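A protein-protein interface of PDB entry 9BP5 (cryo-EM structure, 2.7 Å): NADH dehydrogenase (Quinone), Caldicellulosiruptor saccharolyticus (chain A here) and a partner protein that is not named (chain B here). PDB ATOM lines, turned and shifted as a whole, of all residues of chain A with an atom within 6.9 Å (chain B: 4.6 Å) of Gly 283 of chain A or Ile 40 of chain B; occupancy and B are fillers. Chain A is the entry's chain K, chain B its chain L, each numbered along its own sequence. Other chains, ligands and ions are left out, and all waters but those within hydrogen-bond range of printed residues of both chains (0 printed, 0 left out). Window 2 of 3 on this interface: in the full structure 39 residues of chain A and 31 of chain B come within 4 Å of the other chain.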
ATOM      1  N   LYS A 263       5.393  32.246  -1.862  1.00  0.00           N
ATOM      2  CA  LYS A 263       5.784  30.916  -1.407  1.00  0.00           C
ATOM      3  C   LYS A 263       6.858  31.092  -0.340  1.00  0.00           C
ATOM      4  O   LYS A 263       8.027  31.328  -0.657  1.00  0.00           O
ATOM      5  CB  LYS A 263       6.280  30.063  -2.567  1.00  0.00           C
ATOM      6  CG  LYS A 263       5.818  28.624  -2.506  1.00  0.00           C
ATOM      7  CD  LYS A 263       4.537  28.427  -3.292  1.00  0.00           C
ATOM      8  CE  LYS A 263       4.068  26.986  -3.223  1.00  0.00           C
ATOM      9  NZ  LYS A 263       3.043  26.689  -4.260  1.00  0.00           N
ATOM     10  N   LEU A 277      15.445  25.431  -5.507  1.00  0.00           N
ATOM     11  CA  LEU A 277      14.288  26.303  -5.335  1.00  0.00           C
ATOM     12  C   LEU A 277      13.056  25.716  -6.007  1.00  0.00           C
ATOM     13  O   LEU A 277      11.949  25.776  -5.459  1.00  0.00           O
ATOM     14  CB  LEU A 277      14.589  27.690  -5.899  1.00  0.00           C
ATOM     15  CG  LEU A 277      13.536  28.774  -5.681  1.00  0.00           C
ATOM     16  CD1 LEU A 277      14.205  30.079  -5.314  1.00  0.00           C
ATOM     17  CD2 LEU A 277      12.687  28.950  -6.924  1.00  0.00           C
ATOM     18  N   ILE A 278      13.231  25.150  -7.201  1.00  0.00           N
ATOM     19  CA  ILE A 278      12.121  24.515  -7.901  1.00  0.00           C
ATOM     20  C   ILE A 278      11.577  23.349  -7.088  1.00  0.00           C
ATOM     21  O   ILE A 278      10.359  23.179  -6.953  1.00  0.00           O
ATOM     22  CB  ILE A 278      12.571  24.072  -9.303  1.00  0.00           C
ATOM     23  CG1 ILE A 278      12.687  25.284 -10.222  1.00  0.00           C
ATOM     24  CG2 ILE A 278      11.608  23.057  -9.878  1.00  0.00           C
ATOM     25  CD1 ILE A 278      13.738  25.137 -11.288  1.00  0.00           C
ATOM     26  N   ALA A 279      12.471  22.531  -6.528  1.00  0.00           N
ATOM     27  CA  ALA A 279      12.032  21.410  -5.703  1.00  0.00           C
ATOM     28  C   ALA A 279      11.296  21.890  -4.460  1.00  0.00           C
ATOM     29  O   ALA A 279      10.272  21.314  -4.076  1.00  0.00           O
ATOM     30  CB  ALA A 279      13.228  20.546  -5.316  1.00  0.00           C
ATOM     31  N   SER A 280      11.800  22.945  -3.817  1.00  0.00           N
ATOM     32  CA  SER A 280      11.150  23.468  -2.619  1.00  0.00           C
ATOM     33  C   SER A 280       9.763  24.009  -2.935  1.00  0.00           C
ATOM     34  O   SER A 280       8.824  23.826  -2.153  1.00  0.00           O
ATOM     35  CB  SER A 280      12.011  24.557  -1.984  1.00  0.00           C
ATOM     36  OG  SER A 280      13.093  23.996  -1.265  1.00  0.00           O
ATOM     37  N   ILE A 281       9.618  24.692  -4.071  1.00  0.00           N
ATOM     38  CA  ILE A 281       8.300  25.161  -4.483  1.00  0.00           C
ATOM     39  C   ILE A 281       7.386  23.979  -4.781  1.00  0.00           C
ATOM     40  O   ILE A 281       6.193  24.002  -4.460  1.00  0.00           O
ATOM     41  CB  ILE A 281       8.424  26.109  -5.688  1.00  0.00           C
ATOM     42  CG1 ILE A 281       9.140  27.394  -5.277  1.00  0.00           C
ATOM     43  CG2 ILE A 281       7.061  26.427  -6.258  1.00  0.00           C
ATOM     44  CD1 ILE A 281       9.033  28.506  -6.288  1.00  0.00           C
ATOM     45  N   GLU A 282       7.934  22.920  -5.379  1.00  0.00           N
ATOM     46  CA  GLU A 282       7.146  21.739  -5.703  1.00  0.00           C
ATOM     47  C   GLU A 282       6.713  20.956  -4.474  1.00  0.00           C
ATOM     48  O   GLU A 282       5.891  20.044  -4.605  1.00  0.00           O
ATOM     49  CB  GLU A 282       7.933  20.823  -6.636  1.00  0.00           C
ATOM     50  CG  GLU A 282       7.968  21.292  -8.069  1.00  0.00           C
ATOM     51  CD  GLU A 282       8.717  20.339  -8.968  1.00  0.00           C
ATOM     52  OE1 GLU A 282       9.030  19.220  -8.514  1.00  0.00           O
ATOM     53  OE2 GLU A 282       8.992  20.706 -10.127  1.00  0.00           O
ATOM     54  N   GLY A 283       7.244  21.271  -3.298  1.00  0.00           N
ATOM     55  CA  GLY A 283       6.864  20.589  -2.080  1.00  0.00           C
ATOM     56  C   GLY A 283       7.793  19.481  -1.641  1.00  0.00           C
ATOM     57  O   GLY A 283       7.573  18.906  -0.571  1.00  0.00           O
ATOM     58  N   GLU A 284       8.816  19.162  -2.425  1.00  0.00           N
ATOM     59  CA  GLU A 284       9.792  18.159  -2.040  1.00  0.00           C
ATOM     60  C   GLU A 284      10.924  18.809  -1.246  1.00  0.00           C
ATOM     61  O   GLU A 284      10.941  20.019  -1.015  1.00  0.00           O
ATOM     62  CB  GLU A 284      10.333  17.440  -3.273  1.00  0.00           C
ATOM     63  CG  GLU A 284       9.259  16.911  -4.197  1.00  0.00           C
ATOM     64  CD  GLU A 284       9.698  16.898  -5.644  1.00  0.00           C
ATOM     65  OE1 GLU A 284      10.852  17.289  -5.918  1.00  0.00           O
ATOM     66  OE2 GLU A 284       8.893  16.495  -6.509  1.00  0.00           O
ATOM     67  N   ARG A 285      11.879  17.993  -0.812  1.00  0.00           N
ATOM     68  CA  ARG A 285      13.062  18.530  -0.159  1.00  0.00           C
ATOM     69  C   ARG A 285      13.971  19.182  -1.191  1.00  0.00           C
ATOM     70  O   ARG A 285      14.094  18.707  -2.323  1.00  0.00           O
ATOM     71  CB  ARG A 285      13.806  17.430   0.590  1.00  0.00           C
ATOM     72  CG  ARG A 285      13.988  16.157  -0.201  1.00  0.00           C
ATOM     73  CD  ARG A 285      14.420  15.012   0.696  1.00  0.00           C
ATOM     74  NE  ARG A 285      15.759  15.204   1.238  1.00  0.00           N
ATOM     75  CZ  ARG A 285      16.077  15.042   2.515  1.00  0.00           C
ATOM     76  NH1 ARG A 285      15.169  14.706   3.416  1.00  0.00           N
ATOM     77  NH2 ARG A 285      17.337  15.222   2.899  1.00  0.00           N
ATOM     78  N   TRP A 301       7.131  21.937 -12.101  1.00  0.00           N
ATOM     79  CA  TRP A 301       6.218  20.928 -12.633  1.00  0.00           C
ATOM     80  C   TRP A 301       6.380  20.776 -14.145  1.00  0.00           C
ATOM     81  O   TRP A 301       5.413  20.593 -14.884  1.00  0.00           O
ATOM     82  CB  TRP A 301       4.771  21.253 -12.255  1.00  0.00           C
ATOM     83  CG  TRP A 301       4.571  21.415 -10.779  1.00  0.00           C
ATOM     84  CD1 TRP A 301       4.593  20.429  -9.840  1.00  0.00           C
ATOM     85  CD2 TRP A 301       4.325  22.636 -10.072  1.00  0.00           C
ATOM     86  NE1 TRP A 301       4.372  20.957  -8.592  1.00  0.00           N
ATOM     87  CE2 TRP A 301       4.205  22.312  -8.708  1.00  0.00           C
ATOM     88  CE3 TRP A 301       4.191  23.970 -10.460  1.00  0.00           C
ATOM     89  CZ2 TRP A 301       3.961  23.271  -7.732  1.00  0.00           C
ATOM     90  CZ3 TRP A 301       3.948  24.922  -9.487  1.00  0.00           C
ATOM     91  CH2 TRP A 301       3.837  24.567  -8.141  1.00  0.00           C
ATOM     92  N   SER B  38       1.761  19.556  -3.261  1.00  0.00           N
ATOM     93  CA  SER B  38       2.854  20.510  -3.343  1.00  0.00           C
ATOM     94  C   SER B  38       2.789  21.573  -2.257  1.00  0.00           C
ATOM     95  O   SER B  38       3.649  22.457  -2.222  1.00  0.00           O
ATOM     96  CB  SER B  38       2.859  21.183  -4.718  1.00  0.00           C
ATOM     97  OG  SER B  38       2.081  22.366  -4.703  1.00  0.00           O
ATOM     98  N   ASN B  39       1.791  21.515  -1.377  1.00  0.00           N
ATOM     99  CA  ASN B  39       1.628  22.477  -0.296  1.00  0.00           C
ATOM    100  C   ASN B  39       2.059  21.910   1.047  1.00  0.00           C
ATOM    101  O   ASN B  39       1.704  22.466   2.091  1.00  0.00           O
ATOM    102  CB  ASN B  39       0.175  22.948  -0.225  1.00  0.00           C
ATOM    103  CG  ASN B  39      -0.154  23.987  -1.276  1.00  0.00           C
ATOM    104  OD1 ASN B  39       0.660  24.855  -1.585  1.00  0.00           O
ATOM    105  ND2 ASN B  39      -1.356  23.902  -1.833  1.00  0.00           N
ATOM    106  N   ILE B  40       2.818  20.814   1.042  1.00  0.00           N
ATOM    107  CA  ILE B  40       3.115  20.116   2.287  1.00  0.00           C
ATOM    108  C   ILE B  40       4.024  20.942   3.187  1.00  0.00           C
ATOM    109  O   ILE B  40       3.941  20.841   4.417  1.00  0.00           O
ATOM    110  CB  ILE B  40       3.707  18.727   1.988  1.00  0.00           C
ATOM    111  CG1 ILE B  40       3.449  17.790   3.160  1.00  0.00           C
ATOM    112  CG2 ILE B  40       5.182  18.813   1.681  1.00  0.00           C
ATOM    113  CD1 ILE B  40       2.111  17.119   3.085  1.00  0.00           C
ATOM    114  N   ILE B  41       4.895  21.771   2.612  1.00  0.00           N
ATOM    115  CA  ILE B  41       5.763  22.598   3.442  1.00  0.00           C
ATOM    116  C   ILE B  41       4.952  23.667   4.161  1.00  0.00           C
ATOM    117  O   ILE B  41       5.213  23.984   5.327  1.00  0.00           O
ATOM    118  CB  ILE B  41       6.892  23.210   2.599  1.00  0.00           C
ATOM    119  CG1 ILE B  41       7.395  22.190   1.579  1.00  0.00           C
ATOM    120  CG2 ILE B  41       8.025  23.663   3.496  1.00  0.00           C
ATOM    121  CD1 ILE B  41       8.694  22.573   0.917  1.00  0.00           C
ATOM    122  N   ALA B  42       3.954  24.237   3.484  1.00  0.00           N
ATOM    123  CA  ALA B  42       3.077  25.198   4.144  1.00  0.00           C
ATOM    124  C   ALA B  42       2.275  24.533   5.254  1.00  0.00           C
ATOM    125  O   ALA B  42       2.049  25.131   6.313  1.00  0.00           O
ATOM    126  CB  ALA B  42       2.148  25.848   3.123  1.00  0.00           C
ATOM    127  N   ILE B  43       1.840  23.292   5.030  1.00  0.00           N
ATOM    128  CA  ILE B  43       1.121  22.554   6.064  1.00  0.00           C
ATOM    129  C   ILE B  43       2.021  22.310   7.267  1.00  0.00           C
ATOM    130  O   ILE B  43       1.589  22.436   8.418  1.00  0.00           O
ATOM    131  CB  ILE B  43       0.570  21.238   5.492  1.00  0.00           C
ATOM    132  CG1 ILE B  43      -0.453  21.533   4.406  1.00  0.00           C
ATOM    133  CG2 ILE B  43      -0.065  20.413   6.583  1.00  0.00           C
ATOM    134  CD1 ILE B  43      -0.862  20.325   3.627  1.00  0.00           C
ATOM    135  N   LEU B  44       3.283  21.952   7.025  1.00  0.00           N
ATOM    136  CA  LEU B  44       4.218  21.762   8.130  1.00  0.00           C
ATOM    137  C   LEU B  44       4.467  23.066   8.877  1.00  0.00           C
ATOM    138  O   LEU B  44       4.577  23.073  10.108  1.00  0.00           O
ATOM    139  CB  LEU B  44       5.532  21.178   7.615  1.00  0.00           C
ATOM    140  CG  LEU B  44       5.469  19.745   7.091  1.00  0.00           C
ATOM    141  CD1 LEU B  44       6.804  19.337   6.510  1.00  0.00           C
ATOM    142  CD2 LEU B  44       5.056  18.795   8.192  1.00  0.00           C
ATOM    143  N   ILE B  62      -1.126  14.246   8.712  1.00  0.00           N
ATOM    144  CA  ILE B  62      -0.864  14.963   7.466  1.00  0.00           C
ATOM    145  C   ILE B  62      -0.632  13.979   6.330  1.00  0.00           C
ATOM    146  O   ILE B  62      -1.126  14.171   5.214  1.00  0.00           O
ATOM    147  CB  ILE B  62       0.329  15.922   7.627  1.00  0.00           C
ATOM    148  CG1 ILE B  62       0.039  16.986   8.678  1.00  0.00           C
ATOM    149  CG2 ILE B  62       0.642  16.594   6.316  1.00  0.00           C
ATOM    150  CD1 ILE B  62       1.288  17.542   9.318  1.00  0.00           C
ATOM    151  N   THR B  66      -3.283  14.338   3.291  1.00  0.00           N
ATOM    152  CA  THR B  66      -2.749  14.865   2.041  1.00  0.00           C
ATOM    153  C   THR B  66      -2.469  13.763   1.032  1.00  0.00           C
ATOM    154  O   THR B  66      -2.414  14.030  -0.174  1.00  0.00           O
ATOM    155  CB  THR B  66      -1.472  15.658   2.304  1.00  0.00           C
ATOM    156  OG1 THR B  66      -0.572  14.867   3.088  1.00  0.00           O
ATOM    157  CG2 THR B  66      -1.789  16.929   3.047  1.00  0.00           C
ATOM    158  N   VAL B  68       0.386  12.207   0.941  1.00  0.00           N
ATOM    159  CA  VAL B  68       1.831  12.155   0.765  1.00  0.00           C
ATOM    160  C   VAL B  68       2.401  11.061   1.654  1.00  0.00           C
ATOM    161  O   VAL B  68       1.928  10.841   2.775  1.00  0.00           O
ATOM    162  CB  VAL B  68       2.462  13.519   1.083  1.00  0.00           C
ATOM    163  CG1 VAL B  68       3.864  13.596   0.511  1.00  0.00           C
ATOM    164  CG2 VAL B  68       1.600  14.630   0.527  1.00  0.00           C
ATOM    165  N   ILE B  73       7.299  13.029   4.286  1.00  0.00           N
ATOM    166  CA  ILE B  73       7.005  13.988   5.349  1.00  0.00           C
ATOM    167  C   ILE B  73       8.165  14.061   6.331  1.00  0.00           C
ATOM    168  O   ILE B  73       8.600  15.149   6.729  1.00  0.00           O
ATOM    169  CB  ILE B  73       5.694  13.620   6.065  1.00  0.00           C
ATOM    170  CG1 ILE B  73       4.565  13.409   5.059  1.00  0.00           C
ATOM    171  CG2 ILE B  73       5.318  14.698   7.062  1.00  0.00           C
ATOM    172  CD1 ILE B  73       4.425  14.519   4.065  1.00  0.00           C
ATOM    173  N   ILE B  76      11.221  15.852   4.641  1.00  0.00           N
ATOM    174  CA  ILE B  76      11.100  17.305   4.630  1.00  0.00           C
ATOM    175  C   ILE B  76      11.258  17.865   6.035  1.00  0.00           C
ATOM    176  O   ILE B  76      11.948  18.868   6.243  1.00  0.00           O
ATOM    177  CB  ILE B  76       9.762  17.733   4.004  1.00  0.00           C
ATOM    178  CG1 ILE B  76       9.642  17.204   2.582  1.00  0.00           C
ATOM    179  CG2 ILE B  76       9.639  19.238   4.008  1.00  0.00           C
ATOM    180  CD1 ILE B  76       8.225  17.020   2.137  1.00  0.00           C
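The backbone NH (N) of Glu 284 of chain A is in hydrogen-bond range of the backbone carbonyl oxygen (O) of Ala 279 of chain A, at 3.1 Å. The backbone NH (N) of Trp 301 of chain A lies within hydrogen-bond range of the side-chain carboxylate (OE2) of Glu 282 of chain A.
Among the printed residues, merely in contact across the chains: Ser 280 of chain A with Ile 41 of chain B (3.3 Å), Ile 281 of chain A with Ser 38 of chain B (3.7 Å), Glu 282 of chain A with Ser 38 of chain B (3.2 Å), Gly 283 of chain A with Ser 38 of chain B (3.7 Å), Gly 283 of chain A with Ile 40 of chain B (3.3 Å), Gly 283 of chain A with Ile 41 of chain B (3.9 Å), Gly 283 of chain A with Ile 76 of chain B (3.4 Å), Glu 284 of chain A with Ile 41 of chain B (3.9 Å) and Trp 301 of chain A with Ser 38 of chain B (3.7 Å).
Of chain B, only Ser 38, Ile 40, Ile 41 and Ile 76 come within 4 Å of Gly 283 of chain A. Of chain A, only Gly 283 (3.3 Å) comes within 4 Å of Ile 40 of chain B. Of the printed residues of chain B, Ser 280 of chain A touches Ile 41 (3.3 Å). Of the printed residues of chain B, Glu 282 of chain A touches Ser 38. Of the printed residues of chain A, Ile 41 of chain B touches Ser 280 (3.3 Å), Gly 283 (3.9 Å) and Glu 284 (3.9 Å). Of the printed residues of chain B, Trp 301 of chain A touches Ser 38 (3.7 Å). The nearest printed residue of chain B that does not touch Gly 283 of chain A is Asn 39 of chain B (5.2 Å). The nearest printed residue of chain A that does not touch Ile 76 of chain B is Arg 285 of chain A (4.1 Å).
Of the 12 printed residues of chain B, 4 touch a printed residue of chain A. Of the 11 printed residues of chain A, 6 touch a printed residue of chain B. Along chain A the printed residues that touch a printed residue of chain B span positions 280 to 301.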
